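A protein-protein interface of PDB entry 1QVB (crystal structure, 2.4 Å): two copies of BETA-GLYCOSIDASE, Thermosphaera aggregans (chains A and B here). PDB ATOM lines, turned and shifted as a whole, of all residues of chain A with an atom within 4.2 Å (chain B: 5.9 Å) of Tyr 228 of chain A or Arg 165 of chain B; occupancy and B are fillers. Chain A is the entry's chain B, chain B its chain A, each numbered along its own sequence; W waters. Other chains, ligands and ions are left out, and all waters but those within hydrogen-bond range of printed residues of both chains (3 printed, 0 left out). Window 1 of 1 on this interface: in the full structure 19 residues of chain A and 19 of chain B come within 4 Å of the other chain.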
ATOM      1  N   VAL A 164      -5.659  26.627 -26.682  1.00  0.00           N
ATOM      2  CA  VAL A 164      -6.962  27.278 -26.780  1.00  0.00           C
ATOM      3  C   VAL A 164      -8.063  26.218 -26.857  1.00  0.00           C
ATOM      4  O   VAL A 164      -9.124  26.366 -26.249  1.00  0.00           O
ATOM      5  CB  VAL A 164      -7.055  28.198 -28.046  1.00  0.00           C
ATOM      6  CG1 VAL A 164      -8.487  28.645 -28.278  1.00  0.00           C
ATOM      7  CG2 VAL A 164      -6.181  29.423 -27.869  1.00  0.00           C
ATOM      8  N   GLY A 168      -9.612  26.512 -23.423  1.00  0.00           N
ATOM      9  CA  GLY A 168     -10.574  27.557 -23.704  1.00  0.00           C
ATOM     10  C   GLY A 168      -9.787  28.828 -23.997  1.00  0.00           C
ATOM     11  O   GLY A 168      -8.648  28.977 -23.540  1.00  0.00           O
ATOM     12  N   PRO A 169     -10.371  29.773 -24.743  1.00  0.00           N
ATOM     13  CA  PRO A 169      -9.721  31.035 -25.103  1.00  0.00           C
ATOM     14  C   PRO A 169      -9.231  31.863 -23.920  1.00  0.00           C
ATOM     15  O   PRO A 169      -8.206  32.529 -24.017  1.00  0.00           O
ATOM     16  CB  PRO A 169     -10.814  31.755 -25.892  1.00  0.00           C
ATOM     17  CG  PRO A 169     -11.556  30.606 -26.512  1.00  0.00           C
ATOM     18  CD  PRO A 169     -11.733  29.753 -25.293  1.00  0.00           C
ATOM     19  N   GLY A 216     -11.599  28.806 -38.308  1.00  0.00           N
ATOM     20  CA  GLY A 216     -11.096  28.567 -36.970  1.00  0.00           C
ATOM     21  C   GLY A 216     -12.132  28.467 -35.862  1.00  0.00           C
ATOM     22  O   GLY A 216     -11.919  27.752 -34.866  1.00  0.00           O
ATOM     23  N   TYR A 217     -13.267  29.141 -36.025  1.00  0.00           N
ATOM     24  CA  TYR A 217     -14.271  29.134 -34.973  1.00  0.00           C
ATOM     25  C   TYR A 217     -15.675  28.668 -35.362  1.00  0.00           C
ATOM     26  O   TYR A 217     -16.584  28.642 -34.523  1.00  0.00           O
ATOM     27  CB  TYR A 217     -14.336  30.538 -34.364  1.00  0.00           C
ATOM     28  CG  TYR A 217     -12.991  31.039 -33.882  1.00  0.00           C
ATOM     29  CD1 TYR A 217     -12.408  30.532 -32.721  1.00  0.00           C
ATOM     30  CD2 TYR A 217     -12.280  31.990 -34.611  1.00  0.00           C
ATOM     31  CE1 TYR A 217     -11.160  30.962 -32.301  1.00  0.00           C
ATOM     32  CE2 TYR A 217     -11.025  32.425 -34.200  1.00  0.00           C
ATOM     33  CZ  TYR A 217     -10.474  31.904 -33.042  1.00  0.00           C
ATOM     34  OH  TYR A 217      -9.236  32.311 -32.628  1.00  0.00           O
ATOM     35  N   VAL A 220     -15.125  24.135 -37.980  1.00  0.00           N
ATOM     36  CA  VAL A 220     -14.053  23.393 -37.346  1.00  0.00           C
ATOM     37  C   VAL A 220     -13.657  22.056 -37.981  1.00  0.00           C
ATOM     38  O   VAL A 220     -12.546  21.573 -37.763  1.00  0.00           O
ATOM     39  CB  VAL A 220     -14.364  23.204 -35.833  1.00  0.00           C
ATOM     40  CG1 VAL A 220     -14.513  24.576 -35.171  1.00  0.00           C
ATOM     41  CG2 VAL A 220     -15.637  22.391 -35.641  1.00  0.00           C
ATOM     42  N   PRO A 226      -7.826  27.627 -34.136  1.00  0.00           N
ATOM     43  CA  PRO A 226      -7.590  26.672 -33.055  1.00  0.00           C
ATOM     44  C   PRO A 226      -8.680  25.591 -33.038  1.00  0.00           C
ATOM     45  O   PRO A 226      -8.723  24.749 -32.135  1.00  0.00           O
ATOM     46  CB  PRO A 226      -7.662  27.564 -31.835  1.00  0.00           C
ATOM     47  CG  PRO A 226      -8.899  28.379 -32.183  1.00  0.00           C
ATOM     48  CD  PRO A 226      -8.568  28.797 -33.622  1.00  0.00           C
ATOM     49  N   GLY A 227      -9.562  25.630 -34.029  1.00  0.00           N
ATOM     50  CA  GLY A 227     -10.635  24.652 -34.099  1.00  0.00           C
ATOM     51  C   GLY A 227     -11.524  24.724 -32.874  1.00  0.00           C
ATOM     52  O   GLY A 227     -11.920  23.704 -32.325  1.00  0.00           O
ATOM     53  N   TYR A 228     -11.840  25.941 -32.450  1.00  0.00           N
ATOM     54  CA  TYR A 228     -12.672  26.167 -31.275  1.00  0.00           C
ATOM     55  C   TYR A 228     -14.054  26.684 -31.683  1.00  0.00           C
ATOM     56  O   TYR A 228     -14.261  27.884 -31.870  1.00  0.00           O
ATOM     57  CB  TYR A 228     -11.941  27.148 -30.354  1.00  0.00           C
ATOM     58  CG  TYR A 228     -12.649  27.470 -29.071  1.00  0.00           C
ATOM     59  CD1 TYR A 228     -13.464  28.591 -28.968  1.00  0.00           C
ATOM     60  CD2 TYR A 228     -12.536  26.628 -27.968  1.00  0.00           C
ATOM     61  CE1 TYR A 228     -14.156  28.869 -27.797  1.00  0.00           C
ATOM     62  CE2 TYR A 228     -13.221  26.893 -26.792  1.00  0.00           C
ATOM     63  CZ  TYR A 228     -14.030  28.011 -26.714  1.00  0.00           C
ATOM     64  OH  TYR A 228     -14.725  28.267 -25.558  1.00  0.00           O
ATOM     65  N   LEU A 229     -14.998  25.761 -31.828  1.00  0.00           N
ATOM     66  CA  LEU A 229     -16.354  26.101 -32.249  1.00  0.00           C
ATOM     67  C   LEU A 229     -17.039  27.077 -31.301  1.00  0.00           C
ATOM     68  O   LEU A 229     -17.271  26.770 -30.138  1.00  0.00           O
ATOM     69  CB  LEU A 229     -17.186  24.823 -32.398  1.00  0.00           C
ATOM     70  CG  LEU A 229     -18.637  24.928 -32.873  1.00  0.00           C
ATOM     71  CD1 LEU A 229     -18.711  25.698 -34.195  1.00  0.00           C
ATOM     72  CD2 LEU A 229     -19.217  23.518 -33.031  1.00  0.00           C
ATOM     73  N   SER A 230     -17.360  28.257 -31.817  1.00  0.00           N
ATOM     74  CA  SER A 230     -18.012  29.302 -31.031  1.00  0.00           C
ATOM     75  C   SER A 230     -18.321  30.503 -31.917  1.00  0.00           C
ATOM     76  O   SER A 230     -17.411  31.199 -32.364  1.00  0.00           O
ATOM     77  CB  SER A 230     -17.101  29.750 -29.887  1.00  0.00           C
ATOM     78  OG  SER A 230     -17.650  30.873 -29.221  1.00  0.00           O
ATOM     79  N   TRP B  35     -27.004  18.186 -27.950  1.00  0.00           N
ATOM     80  CA  TRP B  35     -25.958  18.155 -28.965  1.00  0.00           C
ATOM     81  C   TRP B  35     -26.455  18.243 -30.408  1.00  0.00           C
ATOM     82  O   TRP B  35     -25.912  19.020 -31.200  1.00  0.00           O
ATOM     83  CB  TRP B  35     -25.105  16.898 -28.760  1.00  0.00           C
ATOM     84  CG  TRP B  35     -23.915  16.763 -29.662  1.00  0.00           C
ATOM     85  CD1 TRP B  35     -23.827  16.023 -30.808  1.00  0.00           C
ATOM     86  CD2 TRP B  35     -22.632  17.376 -29.482  1.00  0.00           C
ATOM     87  NE1 TRP B  35     -22.567  16.135 -31.348  1.00  0.00           N
ATOM     88  CE2 TRP B  35     -21.815  16.960 -30.554  1.00  0.00           C
ATOM     89  CE3 TRP B  35     -22.092  18.239 -28.514  1.00  0.00           C
ATOM     90  CZ2 TRP B  35     -20.483  17.379 -30.687  1.00  0.00           C
ATOM     91  CZ3 TRP B  35     -20.762  18.653 -28.649  1.00  0.00           C
ATOM     92  CH2 TRP B  35     -19.979  18.223 -29.725  1.00  0.00           C
ATOM     93  N   ASP B  38     -28.062  21.688 -31.226  1.00  0.00           N
ATOM     94  CA  ASP B  38     -27.149  22.819 -31.151  1.00  0.00           C
ATOM     95  C   ASP B  38     -26.921  23.541 -32.485  1.00  0.00           C
ATOM     96  O   ASP B  38     -26.507  22.922 -33.477  1.00  0.00           O
ATOM     97  CB  ASP B  38     -25.805  22.357 -30.608  1.00  0.00           C
ATOM     98  CG  ASP B  38     -24.873  23.505 -30.350  1.00  0.00           C
ATOM     99  OD1 ASP B  38     -25.160  24.274 -29.414  1.00  0.00           O
ATOM    100  OD2 ASP B  38     -23.870  23.653 -31.085  1.00  0.00           O
ATOM    101  N   GLU B  40     -24.593  25.804 -33.367  1.00  0.00           N
ATOM    102  CA  GLU B  40     -23.198  25.780 -33.781  1.00  0.00           C
ATOM    103  C   GLU B  40     -22.799  24.422 -34.363  1.00  0.00           C
ATOM    104  O   GLU B  40     -22.173  24.363 -35.420  1.00  0.00           O
ATOM    105  CB  GLU B  40     -22.302  26.173 -32.605  1.00  0.00           C
ATOM    106  CG  GLU B  40     -22.617  27.568 -32.092  1.00  0.00           C
ATOM    107  CD  GLU B  40     -21.772  27.990 -30.898  1.00  0.00           C
ATOM    108  OE1 GLU B  40     -21.764  27.266 -29.886  1.00  0.00           O
ATOM    109  OE2 GLU B  40     -21.127  29.054 -30.963  1.00  0.00           O
ATOM    110  N   ASN B  41     -23.166  23.331 -33.695  1.00  0.00           N
ATOM    111  CA  ASN B  41     -22.835  22.010 -34.226  1.00  0.00           C
ATOM    112  C   ASN B  41     -23.437  21.836 -35.618  1.00  0.00           C
ATOM    113  O   ASN B  41     -22.818  21.249 -36.504  1.00  0.00           O
ATOM    114  CB  ASN B  41     -23.363  20.887 -33.328  1.00  0.00           C
ATOM    115  CG  ASN B  41     -22.656  20.821 -32.000  1.00  0.00           C
ATOM    116  OD1 ASN B  41     -21.497  21.187 -31.898  1.00  0.00           O
ATOM    117  ND2 ASN B  41     -23.338  20.309 -30.983  1.00  0.00           N
ATOM    118  N   LEU B  46     -21.199  19.314 -37.899  1.00  0.00           N
ATOM    119  CA  LEU B  46     -20.863  18.216 -36.992  1.00  0.00           C
ATOM    120  C   LEU B  46     -22.054  17.268 -36.897  1.00  0.00           C
ATOM    121  O   LEU B  46     -21.886  16.053 -36.838  1.00  0.00           O
ATOM    122  CB  LEU B  46     -20.478  18.750 -35.609  1.00  0.00           C
ATOM    123  CG  LEU B  46     -19.085  19.394 -35.561  1.00  0.00           C
ATOM    124  CD1 LEU B  46     -18.856  20.119 -34.265  1.00  0.00           C
ATOM    125  CD2 LEU B  46     -18.050  18.314 -35.764  1.00  0.00           C
ATOM    126  N   ASN B 160     -22.721  17.799 -19.748  1.00  0.00           N
ATOM    127  CA  ASN B 160     -23.118  18.981 -20.507  1.00  0.00           C
ATOM    128  C   ASN B 160     -22.044  19.069 -21.588  1.00  0.00           C
ATOM    129  O   ASN B 160     -20.999  19.700 -21.398  1.00  0.00           O
ATOM    130  CB  ASN B 160     -23.075  20.239 -19.642  1.00  0.00           C
ATOM    131  CG  ASN B 160     -23.654  21.447 -20.356  1.00  0.00           C
ATOM    132  OD1 ASN B 160     -23.359  21.688 -21.524  1.00  0.00           O
ATOM    133  ND2 ASN B 160     -24.472  22.216 -19.653  1.00  0.00           N
ATOM    134  N   PRO B 161     -22.299  18.459 -22.750  1.00  0.00           N
ATOM    135  CA  PRO B 161     -21.353  18.438 -23.869  1.00  0.00           C
ATOM    136  C   PRO B 161     -20.902  19.793 -24.383  1.00  0.00           C
ATOM    137  O   PRO B 161     -19.713  20.001 -24.610  1.00  0.00           O
ATOM    138  CB  PRO B 161     -22.104  17.631 -24.925  1.00  0.00           C
ATOM    139  CG  PRO B 161     -23.544  18.029 -24.645  1.00  0.00           C
ATOM    140  CD  PRO B 161     -23.551  17.795 -23.149  1.00  0.00           C
ATOM    141  N   ILE B 162     -21.847  20.705 -24.569  1.00  0.00           N
ATOM    142  CA  ILE B 162     -21.522  22.031 -25.076  1.00  0.00           C
ATOM    143  C   ILE B 162     -20.580  22.760 -24.132  1.00  0.00           C
ATOM    144  O   ILE B 162     -19.624  23.387 -24.569  1.00  0.00           O
ATOM    145  CB  ILE B 162     -22.797  22.890 -25.272  1.00  0.00           C
ATOM    146  CG1 ILE B 162     -23.801  22.142 -26.156  1.00  0.00           C
ATOM    147  CG2 ILE B 162     -22.434  24.226 -25.912  1.00  0.00           C
ATOM    148  CD1 ILE B 162     -23.261  21.754 -27.510  1.00  0.00           C
ATOM    149  N   MET B 163     -20.844  22.667 -22.837  1.00  0.00           N
ATOM    150  CA  MET B 163     -20.014  23.343 -21.847  1.00  0.00           C
ATOM    151  C   MET B 163     -18.622  22.705 -21.748  1.00  0.00           C
ATOM    152  O   MET B 163     -17.636  23.395 -21.474  1.00  0.00           O
ATOM    153  CB  MET B 163     -20.725  23.346 -20.485  1.00  0.00           C
ATOM    154  CG  MET B 163     -20.034  24.164 -19.399  1.00  0.00           C
ATOM    155  SD  MET B 163     -20.993  24.240 -17.834  1.00  0.00           S
ATOM    156  CE  MET B 163     -19.867  25.122 -16.807  1.00  0.00           C
ATOM    157  N   VAL B 164     -18.540  21.395 -21.983  1.00  0.00           N
ATOM    158  CA  VAL B 164     -17.261  20.694 -21.946  1.00  0.00           C
ATOM    159  C   VAL B 164     -16.376  21.151 -23.093  1.00  0.00           C
ATOM    160  O   VAL B 164     -15.159  21.258 -22.938  1.00  0.00           O
ATOM    161  CB  VAL B 164     -17.431  19.139 -22.066  1.00  0.00           C
ATOM    162  CG1 VAL B 164     -16.082  18.476 -22.273  1.00  0.00           C
ATOM    163  CG2 VAL B 164     -18.080  18.572 -20.813  1.00  0.00           C
ATOM    164  N   ARG B 165     -16.982  21.420 -24.248  1.00  0.00           N
ATOM    165  CA  ARG B 165     -16.213  21.843 -25.414  1.00  0.00           C
ATOM    166  C   ARG B 165     -15.703  23.280 -25.270  1.00  0.00           C
ATOM    167  O   ARG B 165     -14.558  23.580 -25.616  1.00  0.00           O
ATOM    168  CB  ARG B 165     -17.053  21.745 -26.699  1.00  0.00           C
ATOM    169  CG  ARG B 165     -16.213  21.340 -27.912  1.00  0.00           C
ATOM    170  CD  ARG B 165     -16.669  21.886 -29.283  1.00  0.00           C
ATOM    171  NE  ARG B 165     -18.055  21.624 -29.670  1.00  0.00           N
ATOM    172  CZ  ARG B 165     -19.089  22.380 -29.315  1.00  0.00           C
ATOM    173  NH1 ARG B 165     -18.909  23.454 -28.559  1.00  0.00           N
ATOM    174  NH2 ARG B 165     -20.306  22.081 -29.739  1.00  0.00           N
ATOM    175  N   ARG B 166     -16.558  24.162 -24.762  1.00  0.00           N
ATOM    176  CA  ARG B 166     -16.203  25.570 -24.597  1.00  0.00           C
ATOM    177  C   ARG B 166     -15.270  25.882 -23.443  1.00  0.00           C
ATOM    178  O   ARG B 166     -14.354  26.688 -23.585  1.00  0.00           O
ATOM    179  CB  ARG B 166     -17.455  26.426 -24.394  1.00  0.00           C
ATOM    180  CG  ARG B 166     -18.417  26.481 -25.549  1.00  0.00           C
ATOM    181  CD  ARG B 166     -19.603  27.355 -25.164  1.00  0.00           C
ATOM    182  NE  ARG B 166     -20.573  27.504 -26.244  1.00  0.00           N
ATOM    183  CZ  ARG B 166     -21.741  28.129 -26.120  1.00  0.00           C
ATOM    184  NH1 ARG B 166     -22.089  28.669 -24.957  1.00  0.00           N
ATOM    185  NH2 ARG B 166     -22.567  28.211 -27.157  1.00  0.00           N
ATOM    186  N   MET B 167     -15.511  25.250 -22.299  1.00  0.00           N
ATOM    187  CA  MET B 167     -14.737  25.537 -21.101  1.00  0.00           C
ATOM    188  C   MET B 167     -13.663  24.528 -20.767  1.00  0.00           C
ATOM    189  O   MET B 167     -12.680  24.856 -20.113  1.00  0.00           O
ATOM    190  CB  MET B 167     -15.692  25.657 -19.913  1.00  0.00           C
ATOM    191  CG  MET B 167     -16.879  26.570 -20.168  1.00  0.00           C
ATOM    192  SD  MET B 167     -16.364  28.272 -20.462  1.00  0.00           S
ATOM    193  CE  MET B 167     -15.676  28.687 -18.827  1.00  0.00           C
ATOM    194  N   GLY B 168     -13.846  23.295 -21.209  1.00  0.00           N
ATOM    195  CA  GLY B 168     -12.878  22.264 -20.887  1.00  0.00           C
ATOM    196  C   GLY B 168     -13.547  21.319 -19.906  1.00  0.00           C
ATOM    197  O   GLY B 168     -14.445  21.736 -19.173  1.00  0.00           O
ATOM    198  N   PRO B 226     -18.548  14.970 -26.507  1.00  0.00           N
ATOM    199  CA  PRO B 226     -18.566  16.433 -26.469  1.00  0.00           C
ATOM    200  C   PRO B 226     -17.657  16.999 -27.557  1.00  0.00           C
ATOM    201  O   PRO B 226     -17.420  18.206 -27.628  1.00  0.00           O
ATOM    202  CB  PRO B 226     -18.020  16.713 -25.086  1.00  0.00           C
ATOM    203  CG  PRO B 226     -16.865  15.754 -25.071  1.00  0.00           C
ATOM    204  CD  PRO B 226     -17.535  14.462 -25.566  1.00  0.00           C
ATOM    205  N   GLY B 227     -17.134  16.115 -28.398  1.00  0.00           N
ATOM    206  CA  GLY B 227     -16.251  16.549 -29.467  1.00  0.00           C
ATOM    207  C   GLY B 227     -15.043  17.280 -28.915  1.00  0.00           C
ATOM    208  O   GLY B 227     -14.624  18.294 -29.450  1.00  0.00           O
ATOM    209  N   TYR B 228     -14.482  16.747 -27.837  1.00  0.00           N
ATOM    210  CA  TYR B 228     -13.333  17.355 -27.194  1.00  0.00           C
ATOM    211  C   TYR B 228     -12.085  16.511 -27.459  1.00  0.00           C
ATOM    212  O   TYR B 228     -11.810  15.533 -26.757  1.00  0.00           O
ATOM    213  CB  TYR B 228     -13.637  17.501 -25.698  1.00  0.00           C
ATOM    214  CG  TYR B 228     -12.544  18.113 -24.874  1.00  0.00           C
ATOM    215  CD1 TYR B 228     -11.602  17.316 -24.232  1.00  0.00           C
ATOM    216  CD2 TYR B 228     -12.418  19.497 -24.778  1.00  0.00           C
ATOM    217  CE1 TYR B 228     -10.549  17.885 -23.508  1.00  0.00           C
ATOM    218  CE2 TYR B 228     -11.370  20.080 -24.062  1.00  0.00           C
ATOM    219  CZ  TYR B 228     -10.440  19.266 -23.433  1.00  0.00           C
ATOM    220  OH  TYR B 228      -9.393  19.829 -22.744  1.00  0.00           O
HETATM  221  O   HOH W   1     -16.371  25.159 -28.160  1.00  0.00           O
HETATM  222  O   HOH W   2     -20.748  31.080 -28.980  1.00  0.00           O
HETATM  223  O   HOH W   3     -19.507  27.006 -28.682  1.00  0.00           O
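The side-chain hydroxyl (OH) of Tyr 228 of chain A is in hydrogen-bond range of the backbone carbonyl oxygen (O) of Arg 166 of chain B, 2.6 Å away.
The backbone NH (N) of Glu 40 of chain B lies within hydrogen-bond range of the side-chain carboxylate (OD2) of Asp 38 of chain B (3.2 Å). The side-chain carboxylate (OD2) of Asp 38 of chain B sits at hydrogen-bond distance from the backbone NH (N) of Asn 41 of chain B, 2.7 Å away. OE1 of Glu 40 of chain B is in salt-bridge range of NH2 of Arg 166 of chain B, 3.0 Å away. The backbone carbonyl oxygen (O) of Asn 41 of chain B lies within hydrogen-bond range of the backbone NH (N) of Leu 46 of chain B, at 2.9 Å. The backbone carbonyl oxygen of Gly 216 of chain A is in hydrogen-bond range of the backbone NH of Tyr 228 of chain A. The backbone NH of Ser 230 of chain A is in hydrogen-bond range of the backbone carbonyl oxygen of Tyr 217 of chain A (2.8 Å).
Arg 166 of chain B touches Gly 168 of chain A. Tyr 228 of chain A touches Arg 165 of chain B (CE2 to O, 3.8 Å). Glu 40 of chain B touches Leu 229 of chain A. CD2 of Leu 229 of chain A touches OD1 of Asn 41 of chain B, at 3.5 Å. Leu 229 of chain A touches Leu 46 of chain B. Arg 165 of chain B touches Leu 229 of chain A (NH2 to CD2, 3.8 Å). OE2 of Glu 40 of chain B touches CA of Ser 230 of chain A, at 3.1 Å.
Of the printed residues of chain B, Gly 168 of chain A touches Arg 166 (3.9 Å). Of chain B, only Arg 165 (3.8 Å) and Arg 166 (2.6 Å) come within 4 Å of Tyr 228 of chain A. Printed residues of chain A within 4 Å of Leu 46 of chain B: Leu 229. Asn 160 of chain B touches none of the printed residues of chain A. Met 163 of chain B touches none of the printed residues of chain A. The nearest residue of chain B that does not touch Tyr 228 of chain A is Met 167 of chain B (4.5 Å). The nearest printed residue of chain A that does not touch Arg 165 of chain B is Gly 227 of chain A (5.9 Å). The nearest printed residue of chain A that does not touch Leu 46 of chain B is Val 220 of chain A (4.2 Å).
Of the 11 printed residues of chain A, 4 touch a printed residue of chain B. Hydrophobic or aromatic side chains of chain A that line the printed part of chain B: Tyr 228 and Leu 229. Of the 17 printed residues of chain B, 5 touch a printed residue of chain A. Among the printed residues, no Asp or Glu carboxylate lies within 4 Å of a Lys or Arg side-chain nitrogen of the other chain.
Positions printed for both chains: 164, 168, 226, 227 and 228. Of the 8 pairs that touch across the chains among the printed residues, none has its exchanged pair printed and touching as well.
Water W3 lies within hydrogen-bond range of the side-chain carboxylate of Glu 40 of chain B, the backbone carbonyl oxygen of Leu 229 of chain A and the guanidinium group of Arg 166 of chain B. Water W1 bridges O of Leu 229 of chain A and NH1 of Arg 165 of chain B. Water W2 lies within hydrogen-bond range of the side-chain carboxylate (OE2) of Glu 40 of chain B (2.9 Å) and the side-chain hydroxyl (OG) of Ser 230 of chain A (3.1 Å).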
